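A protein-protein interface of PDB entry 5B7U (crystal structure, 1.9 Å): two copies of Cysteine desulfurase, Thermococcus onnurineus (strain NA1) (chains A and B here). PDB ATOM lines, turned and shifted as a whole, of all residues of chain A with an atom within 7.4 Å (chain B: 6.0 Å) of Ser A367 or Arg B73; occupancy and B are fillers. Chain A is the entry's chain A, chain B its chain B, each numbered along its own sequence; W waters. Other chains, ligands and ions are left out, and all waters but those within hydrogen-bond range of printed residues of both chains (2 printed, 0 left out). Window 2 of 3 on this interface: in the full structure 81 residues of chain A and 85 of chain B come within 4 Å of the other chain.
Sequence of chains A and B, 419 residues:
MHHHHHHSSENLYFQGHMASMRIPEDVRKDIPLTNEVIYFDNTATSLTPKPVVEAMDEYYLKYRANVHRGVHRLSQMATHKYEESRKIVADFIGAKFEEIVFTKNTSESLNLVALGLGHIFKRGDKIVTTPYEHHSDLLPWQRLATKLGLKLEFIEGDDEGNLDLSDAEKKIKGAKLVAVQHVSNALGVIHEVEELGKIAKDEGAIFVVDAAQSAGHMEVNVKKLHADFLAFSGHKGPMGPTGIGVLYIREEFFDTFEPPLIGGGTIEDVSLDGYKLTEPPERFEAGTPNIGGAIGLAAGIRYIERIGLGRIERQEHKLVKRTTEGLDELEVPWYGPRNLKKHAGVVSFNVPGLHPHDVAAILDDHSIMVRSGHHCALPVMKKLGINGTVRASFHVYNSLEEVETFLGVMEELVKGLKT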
ATOM      1  N   GLU A  36       7.203 -18.437   2.795  1.00  0.00           N
ATOM      2  CA  GLU A  36       8.273 -17.882   1.988  1.00  0.00           C
ATOM      3  C   GLU A  36       8.986 -16.648   2.520  1.00  0.00           C
ATOM      4  O   GLU A  36      10.118 -16.490   2.265  1.00  0.00           O
ATOM      5  CB  GLU A  36       7.817 -17.539   0.557  1.00  0.00           C
ATOM      6  CG  GLU A  36       7.032 -18.597  -0.154  1.00  0.00           C
ATOM      7  CD  GLU A  36       7.822 -19.854  -0.348  1.00  0.00           C
ATOM      8  OE1 GLU A  36       7.212 -20.915  -0.392  1.00  0.00           O
ATOM      9  OE2 GLU A  36       9.042 -19.779  -0.462  1.00  0.00           O
ATOM     10  N   VAL A  37       8.285 -15.784   3.221  1.00  0.00           N
ATOM     11  CA  VAL A  37       8.863 -14.593   3.755  1.00  0.00           C
ATOM     12  C   VAL A  37       8.278 -14.281   5.145  1.00  0.00           C
ATOM     13  O   VAL A  37       7.310 -14.798   5.497  1.00  0.00           O
ATOM     14  CB  VAL A  37       8.517 -13.392   2.861  1.00  0.00           C
ATOM     15  CG1 VAL A  37       8.984 -13.579   1.431  1.00  0.00           C
ATOM     16  CG2 VAL A  37       7.022 -13.164   2.844  1.00  0.00           C
ATOM     17  N   ILE A  38       8.923 -13.407   5.874  1.00  0.00           N
ATOM     18  CA  ILE A  38       8.430 -12.934   7.136  1.00  0.00           C
ATOM     19  C   ILE A  38       7.821 -11.603   6.718  1.00  0.00           C
ATOM     20  O   ILE A  38       8.515 -10.682   6.435  1.00  0.00           O
ATOM     21  CB  ILE A  38       9.572 -12.721   8.136  1.00  0.00           C
ATOM     22  CG1 ILE A  38      10.163 -14.077   8.558  1.00  0.00           C
ATOM     23  CG2 ILE A  38       9.096 -11.913   9.321  1.00  0.00           C
ATOM     24  CD1 ILE A  38      11.366 -13.990   9.453  1.00  0.00           C
ATOM     25  N   TYR A  39       6.510 -11.557   6.637  1.00  0.00           N
ATOM     26  CA  TYR A  39       5.804 -10.364   6.137  1.00  0.00           C
ATOM     27  C   TYR A  39       5.390  -9.451   7.306  1.00  0.00           C
ATOM     28  O   TYR A  39       4.429  -9.775   8.009  1.00  0.00           O
ATOM     29  CB  TYR A  39       4.533 -10.789   5.405  1.00  0.00           C
ATOM     30  CG  TYR A  39       3.888  -9.625   4.705  1.00  0.00           C
ATOM     31  CD1 TYR A  39       4.270  -9.259   3.435  1.00  0.00           C
ATOM     32  CD2 TYR A  39       2.781  -8.968   5.268  1.00  0.00           C
ATOM     33  CE1 TYR A  39       3.657  -8.184   2.785  1.00  0.00           C
ATOM     34  CE2 TYR A  39       2.178  -7.913   4.628  1.00  0.00           C
ATOM     35  CZ  TYR A  39       2.549  -7.565   3.381  1.00  0.00           C
ATOM     36  OH  TYR A  39       2.013  -6.514   2.728  1.00  0.00           O
ATOM     37  N   PHE A  40       6.130  -8.368   7.473  1.00  0.00           N
ATOM     38  CA  PHE A  40       5.896  -7.350   8.513  1.00  0.00           C
ATOM     39  C   PHE A  40       5.534  -6.038   7.881  1.00  0.00           C
ATOM     40  O   PHE A  40       6.020  -4.982   8.311  1.00  0.00           O
ATOM     41  CB  PHE A  40       7.171  -7.166   9.377  1.00  0.00           C
ATOM     42  CG  PHE A  40       7.474  -8.290  10.366  1.00  0.00           C
ATOM     43  CD1 PHE A  40       6.634  -9.399  10.601  1.00  0.00           C
ATOM     44  CD2 PHE A  40       8.640  -8.200  11.110  1.00  0.00           C
ATOM     45  CE1 PHE A  40       6.941 -10.339  11.597  1.00  0.00           C
ATOM     46  CE2 PHE A  40       8.973  -9.156  12.030  1.00  0.00           C
ATOM     47  CZ  PHE A  40       8.140 -10.225  12.283  1.00  0.00           C
ATOM     48  N   ALA A 360      15.729  -1.320   5.391  1.00  0.00           N
ATOM     49  CA  ALA A 360      14.707  -2.149   4.787  1.00  0.00           C
ATOM     50  C   ALA A 360      15.287  -3.110   3.736  1.00  0.00           C
ATOM     51  O   ALA A 360      14.819  -4.236   3.571  1.00  0.00           O
ATOM     52  CB  ALA A 360      13.592  -1.281   4.164  1.00  0.00           C
ATOM     53  N   ALA A 361      16.257  -2.639   2.999  1.00  0.00           N
ATOM     54  CA  ALA A 361      16.990  -3.437   2.006  1.00  0.00           C
ATOM     55  C   ALA A 361      17.716  -4.618   2.625  1.00  0.00           C
ATOM     56  O   ALA A 361      17.616  -5.747   2.118  1.00  0.00           O
ATOM     57  CB  ALA A 361      17.979  -2.581   1.221  1.00  0.00           C
ATOM     58  N   ILE A 362      18.364  -4.373   3.761  1.00  0.00           N
ATOM     59  CA  ILE A 362      19.038  -5.476   4.487  1.00  0.00           C
ATOM     60  C   ILE A 362      18.039  -6.485   4.969  1.00  0.00           C
ATOM     61  O   ILE A 362      18.216  -7.705   4.821  1.00  0.00           O
ATOM     62  CB  ILE A 362      19.949  -4.934   5.615  1.00  0.00           C
ATOM     63  CG1 ILE A 362      21.091  -4.166   4.963  1.00  0.00           C
ATOM     64  CG2 ILE A 362      20.449  -6.077   6.507  1.00  0.00           C
ATOM     65  CD1 ILE A 362      21.742  -3.169   5.881  1.00  0.00           C
ATOM     66  N   LEU A 363      16.884  -5.991   5.441  1.00  0.00           N
ATOM     67  CA  LEU A 363      15.893  -6.874   5.948  1.00  0.00           C
ATOM     68  C   LEU A 363      15.334  -7.711   4.820  1.00  0.00           C
ATOM     69  O   LEU A 363      15.084  -8.898   5.009  1.00  0.00           O
ATOM     70  CB  LEU A 363      14.763  -6.117   6.711  1.00  0.00           C
ATOM     71  CG  LEU A 363      15.331  -5.649   8.077  1.00  0.00           C
ATOM     72  CD1 LEU A 363      14.570  -4.557   8.789  1.00  0.00           C
ATOM     73  CD2 LEU A 363      15.465  -6.845   9.011  1.00  0.00           C
ATOM     74  N   ASP A 364      15.112  -7.065   3.694  1.00  0.00           N
ATOM     75  CA  ASP A 364      14.661  -7.793   2.498  1.00  0.00           C
ATOM     76  C   ASP A 364      15.634  -8.884   2.043  1.00  0.00           C
ATOM     77  O   ASP A 364      15.202  -9.970   1.649  1.00  0.00           O
ATOM     78  CB  ASP A 364      14.371  -6.851   1.343  1.00  0.00           C
ATOM     79  CG  ASP A 364      13.952  -7.590   0.065  1.00  0.00           C
ATOM     80  OD1 ASP A 364      12.921  -8.359  -0.016  1.00  0.00           O
ATOM     81  OD2 ASP A 364      14.729  -7.438  -0.869  1.00  0.00           O
ATOM     82  N   ASP A 365      16.919  -8.601   2.087  1.00  0.00           N
ATOM     83  CA  ASP A 365      17.924  -9.657   1.774  1.00  0.00           C
ATOM     84  C   ASP A 365      17.695 -10.927   2.625  1.00  0.00           C
ATOM     85  O   ASP A 365      17.881 -12.037   2.155  1.00  0.00           O
ATOM     86  CB  ASP A 365      19.345  -9.172   2.107  1.00  0.00           C
ATOM     87  CG  ASP A 365      19.794  -7.999   1.301  1.00  0.00           C
ATOM     88  OD1 ASP A 365      19.283  -7.784   0.176  1.00  0.00           O
ATOM     89  OD2 ASP A 365      20.715  -7.291   1.805  1.00  0.00           O
ATOM     90  N   HIS A 366      17.304 -10.726   3.903  1.00  0.00           N
ATOM     91  CA  HIS A 366      16.914 -11.820   4.814  1.00  0.00           C
ATOM     92  C   HIS A 366      15.476 -12.269   4.738  1.00  0.00           C
ATOM     93  O   HIS A 366      15.002 -12.924   5.624  1.00  0.00           O
ATOM     94  CB  HIS A 366      17.275 -11.392   6.272  1.00  0.00           C
ATOM     95  CG  HIS A 366      18.749 -11.243   6.503  1.00  0.00           C
ATOM     96  ND1 HIS A 366      19.481 -10.145   6.106  1.00  0.00           N
ATOM     97  CD2 HIS A 366      19.616 -12.060   7.118  1.00  0.00           C
ATOM     98  CE1 HIS A 366      20.739 -10.284   6.496  1.00  0.00           C
ATOM     99  NE2 HIS A 366      20.842 -11.443   7.083  1.00  0.00           N
ATOM    100  N   SER A 367      14.782 -11.949   3.654  1.00  0.00           N
ATOM    101  CA  SER A 367      13.411 -12.293   3.484  1.00  0.00           C
ATOM    102  C   SER A 367      12.434 -11.773   4.573  1.00  0.00           C
ATOM    103  O   SER A 367      11.396 -12.387   4.807  1.00  0.00           O
ATOM    104  CB  SER A 367      13.254 -13.793   3.278  1.00  0.00           C
ATOM    105  OG  SER A 367      13.897 -14.086   2.059  1.00  0.00           O
ATOM    106  N   ILE A 368      12.722 -10.601   5.067  1.00  0.00           N
ATOM    107  CA  ILE A 368      11.885  -9.912   5.999  1.00  0.00           C
ATOM    108  C   ILE A 368      11.383  -8.652   5.305  1.00  0.00           C
ATOM    109  O   ILE A 368      12.136  -7.812   4.940  1.00  0.00           O
ATOM    110  CB  ILE A 368      12.657  -9.526   7.266  1.00  0.00           C
ATOM    111  CG1 ILE A 368      13.137 -10.764   8.007  1.00  0.00           C
ATOM    112  CG2 ILE A 368      11.805  -8.716   8.184  1.00  0.00           C
ATOM    113  CD1 ILE A 368      14.087 -10.452   9.125  1.00  0.00           C
ATOM    114  N   MET A 369      10.078  -8.587   5.143  1.00  0.00           N
ATOM    115  CA  MET A 369       9.420  -7.502   4.462  1.00  0.00           C
ATOM    116  C   MET A 369       8.934  -6.403   5.401  1.00  0.00           C
ATOM    117  O   MET A 369       8.016  -6.604   6.136  1.00  0.00           O
ATOM    118  CB  MET A 369       8.224  -8.016   3.654  1.00  0.00           C
ATOM    119  CG  MET A 369       8.413  -9.340   2.959  1.00  0.00           C
ATOM    120  SD  MET A 369       9.346  -9.279   1.435  1.00  0.00           S
ATOM    121  CE  MET A 369      10.945  -9.792   2.009  1.00  0.00           C
ATOM    122  N   VAL A 370       9.564  -5.249   5.332  1.00  0.00           N
ATOM    123  CA  VAL A 370       9.161  -4.095   6.102  1.00  0.00           C
ATOM    124  C   VAL A 370       9.041  -2.894   5.154  1.00  0.00           C
ATOM    125  O   VAL A 370       9.497  -2.956   4.049  1.00  0.00           O
ATOM    126  CB  VAL A 370      10.196  -3.736   7.191  1.00  0.00           C
ATOM    127  CG1 VAL A 370      10.299  -4.796   8.254  1.00  0.00           C
ATOM    128  CG2 VAL A 370      11.528  -3.422   6.590  1.00  0.00           C
ATOM    129  N   THR A 405      13.648 -14.016  14.670  1.00  0.00           N
ATOM    130  CA  THR A 405      14.489 -13.977  13.474  1.00  0.00           C
ATOM    131  C   THR A 405      14.832 -12.581  13.102  1.00  0.00           C
ATOM    132  O   THR A 405      15.968 -12.247  12.936  1.00  0.00           O
ATOM    133  CB  THR A 405      13.795 -14.721  12.316  1.00  0.00           C
ATOM    134  OG1 THR A 405      13.540 -16.059  12.733  1.00  0.00           O
ATOM    135  CG2 THR A 405      14.578 -14.606  10.980  1.00  0.00           C
ATOM    136  N   VAL A 409      18.397 -10.605  12.984  1.00  0.00           N
ATOM    137  CA  VAL A 409      18.919  -9.898  11.876  1.00  0.00           C
ATOM    138  C   VAL A 409      19.283  -8.471  12.273  1.00  0.00           C
ATOM    139  O   VAL A 409      20.336  -7.928  11.851  1.00  0.00           O
ATOM    140  CB  VAL A 409      17.969  -9.978  10.625  1.00  0.00           C
ATOM    141  CG1 VAL A 409      18.479  -9.103   9.468  1.00  0.00           C
ATOM    142  CG2 VAL A 409      17.789 -11.421  10.194  1.00  0.00           C
ATOM    143  N   GLY B  70       8.039  -0.025  -2.917  1.00  0.00           N
ATOM    144  CA  GLY B  70       8.571  -0.326  -1.623  1.00  0.00           C
ATOM    145  C   GLY B  70       9.871  -1.101  -1.838  1.00  0.00           C
ATOM    146  O   GLY B  70      10.056  -1.717  -2.852  1.00  0.00           O
ATOM    147  N   VAL B  71      10.747  -1.046  -0.859  1.00  0.00           N
ATOM    148  CA  VAL B  71      12.005  -1.705  -0.988  1.00  0.00           C
ATOM    149  C   VAL B  71      11.859  -3.209  -1.110  1.00  0.00           C
ATOM    150  O   VAL B  71      12.528  -3.804  -1.871  1.00  0.00           O
ATOM    151  CB  VAL B  71      12.927  -1.355   0.191  1.00  0.00           C
ATOM    152  CG1 VAL B  71      14.169  -2.201   0.213  1.00  0.00           C
ATOM    153  CG2 VAL B  71      13.300   0.088   0.108  1.00  0.00           C
ATOM    154  N   HIS B  72      10.980  -3.790  -0.340  1.00  0.00           N
ATOM    155  CA  HIS B  72      10.864  -5.216  -0.338  1.00  0.00           C
ATOM    156  C   HIS B  72      10.433  -5.834  -1.633  1.00  0.00           C
ATOM    157  O   HIS B  72       9.761  -5.266  -2.394  1.00  0.00           O
ATOM    158  CB  HIS B  72      10.140  -5.750   0.890  1.00  0.00           C
ATOM    159  CG  HIS B  72       8.672  -5.454   0.942  1.00  0.00           C
ATOM    160  ND1 HIS B  72       7.763  -6.045   0.113  1.00  0.00           N
ATOM    161  CD2 HIS B  72       7.954  -4.696   1.795  1.00  0.00           C
ATOM    162  CE1 HIS B  72       6.559  -5.643   0.425  1.00  0.00           C
ATOM    163  NE2 HIS B  72       6.643  -4.844   1.461  1.00  0.00           N
ATOM    164  N   ARG B  73      10.868  -7.049  -1.819  1.00  0.00           N
ATOM    165  CA  ARG B  73      10.649  -7.759  -3.030  1.00  0.00           C
ATOM    166  C   ARG B  73       9.232  -7.967  -3.493  1.00  0.00           C
ATOM    167  O   ARG B  73       8.981  -8.015  -4.664  1.00  0.00           O
ATOM    168  CB  ARG B  73      11.406  -9.036  -3.017  1.00  0.00           C
ATOM    169  CG  ARG B  73      10.937 -10.009  -2.016  1.00  0.00           C
ATOM    170  CD  ARG B  73      11.471 -11.260  -2.603  1.00  0.00           C
ATOM    171  NE  ARG B  73      11.639 -12.347  -1.718  1.00  0.00           N
ATOM    172  CZ  ARG B  73      12.747 -12.667  -1.082  1.00  0.00           C
ATOM    173  NH1 ARG B  73      13.839 -11.923  -1.128  1.00  0.00           N
ATOM    174  NH2 ARG B  73      12.724 -13.754  -0.358  1.00  0.00           N
ATOM    175  N   LEU B  74       8.346  -8.116  -2.540  1.00  0.00           N
ATOM    176  CA  LEU B  74       6.951  -8.268  -2.863  1.00  0.00           C
ATOM    177  C   LEU B  74       6.437  -6.953  -3.439  1.00  0.00           C
ATOM    178  O   LEU B  74       5.794  -6.953  -4.391  1.00  0.00           O
ATOM    179  CB  LEU B  74       6.149  -8.692  -1.652  1.00  0.00           C
ATOM    180  CG  LEU B  74       6.417 -10.084  -1.093  1.00  0.00           C
ATOM    181  CD1 LEU B  74       5.479 -10.503  -0.011  1.00  0.00           C
ATOM    182  CD2 LEU B  74       6.488 -11.137  -2.129  1.00  0.00           C
ATOM    183  N   SER B  75       6.742  -5.846  -2.816  1.00  0.00           N
ATOM    184  CA  SER B  75       6.336  -4.560  -3.328  1.00  0.00           C
ATOM    185  C   SER B  75       7.007  -4.277  -4.666  1.00  0.00           C
ATOM    186  O   SER B  75       6.412  -3.712  -5.563  1.00  0.00           O
ATOM    187  CB  SER B  75       6.678  -3.429  -2.345  1.00  0.00           C
ATOM    188  OG  SER B  75       6.092  -2.202  -2.805  1.00  0.00           O
ATOM    189  N   GLN B  76       8.252  -4.682  -4.816  1.00  0.00           N
ATOM    190  CA  GLN B  76       8.930  -4.489  -6.104  1.00  0.00           C
ATOM    191  C   GLN B  76       8.159  -5.255  -7.228  1.00  0.00           C
ATOM    192  O   GLN B  76       7.950  -4.759  -8.305  1.00  0.00           O
ATOM    193  CB  GLN B  76      10.394  -4.994  -6.006  1.00  0.00           C
ATOM    194  CG  GLN B  76      11.269  -4.038  -5.199  1.00  0.00           C
ATOM    195  CD  GLN B  76      11.516  -2.766  -5.936  1.00  0.00           C
ATOM    196  OE1 GLN B  76      11.958  -2.789  -7.083  1.00  0.00           O
ATOM    197  NE2 GLN B  76      11.222  -1.648  -5.313  1.00  0.00           N
ATOM    198  N   MET B  77       7.755  -6.470  -6.957  1.00  0.00           N
ATOM    199  CA  MET B  77       7.031  -7.254  -7.925  1.00  0.00           C
ATOM    200  C   MET B  77       5.598  -6.707  -8.195  1.00  0.00           C
ATOM    201  O   MET B  77       5.167  -6.576  -9.333  1.00  0.00           O
ATOM    202  CB  MET B  77       7.043  -8.718  -7.503  1.00  0.00           C
ATOM    203  CG  MET B  77       6.390  -9.707  -8.497  1.00  0.00           C
ATOM    204  SD  MET B  77       6.919  -9.613 -10.254  1.00  0.00           S
ATOM    205  CE  MET B  77       6.017 -11.037 -10.911  1.00  0.00           C
ATOM    206  N   ALA B  78       4.870  -6.397  -7.146  1.00  0.00           N
ATOM    207  CA  ALA B  78       3.565  -5.826  -7.299  1.00  0.00           C
ATOM    208  C   ALA B  78       3.644  -4.518  -8.069  1.00  0.00           C
ATOM    209  O   ALA B  78       2.830  -4.272  -8.954  1.00  0.00           O
ATOM    210  CB  ALA B  78       2.950  -5.608  -5.889  1.00  0.00           C
HETATM  211  O   HOH W   1       3.260  -4.425   1.215  1.00  0.00           O
HETATM  212  O   HOH W   2      13.589  -6.392  -3.304  1.00  0.00           O
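The side-chain carboxylate of Asp A364 is in salt-bridge range of the guanidinium group of Arg B73, at 3.8 Å.
The side-chain hydroxyl (OG) of Ser A367 is in hydrogen-bond range of the guanidinium group (NH2) of Arg B73.
The backbone carbonyl oxygen (O) of Ser A367 sits at hydrogen-bond distance from the backbone NH (N) of Ile A38 (2.9 Å).
O of Ile A38 lies within hydrogen-bond range of N of Met A369, 2.9 Å away.
The backbone NH (N) of Phe A40 lies within hydrogen-bond range of the backbone carbonyl oxygen (O) of Met A369, 2.9 Å away.
N of Leu B74 sits close to ND1 of His B72, 3.4 Å away.
The backbone NH (N) of Ser B75 sits at hydrogen-bond distance from a ring nitrogen (ND1) of His B72.
Among the printed residues, pairs that only touch across the chains: Val A370 with His B72 (3.2 Å), Ala A361 with Val B71 (3.5 Å), Met A369 with His B72 (3.7 Å), Asp A364 with His B72 (3.8 Å), Ala A360 with Val B71 (3.8 Å), Tyr A39 with Leu B74 (3.9 Å), Met A369 with Arg B73 (3.9 Å) and Met A369 with Leu B74 (3.95 Å).
Of the printed residues of chain B, Ala A360 touches Val B71.
Leu A363 touches none of the printed residues of chain B.
Of the printed residues of chain B, Asp A364 touches His B72 and Arg B73.
Printed residues of chain B within 4 Å of Ser A367: Arg B73.
Of the printed residues of chain B, Met A369 touches His B72 (3.7 Å), Arg B73 (3.9 Å) and Leu B74 (3.95 Å).
Printed residues of chain B within 4 Å of Val A370: His B72.
Val A409 touches none of the printed residues of chain B.
Arg B73 touches just these residues of chain A: Asp A364, Ser A367 and Met A369.
The nearest printed residue of chain B that does not touch Ser A367 is His B72 (7.4 Å).
The nearest residue of chain A that does not touch Arg B73 is Val A37 (4.1 Å).
Hydrophobic or aromatic side chains of chain B that line the printed part of chain A: Val B71, His B72 and Leu B74.
Hydrophobic or aromatic side chains of chain A that line the printed part of chain B: Tyr A39, Ala A361 and Met A369.
Among the printed residues, 10 pairs touch across the chains.
No position is printed for both chains.
Of the 10 pairs that touch across the chains among the printed residues, none has its exchanged pair printed and touching as well.
Water W1 bridges OH of Tyr A39 (2.9 Å) and NE2 of His B72 (3.4 Å).
Water W2 lies within hydrogen-bond range of the side-chain carboxylate of Asp A364 (2.9 Å), the backbone carbonyl oxygen of Val B71 (3.1 Å) and the backbone NH of Arg B73 (3.2 Å).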
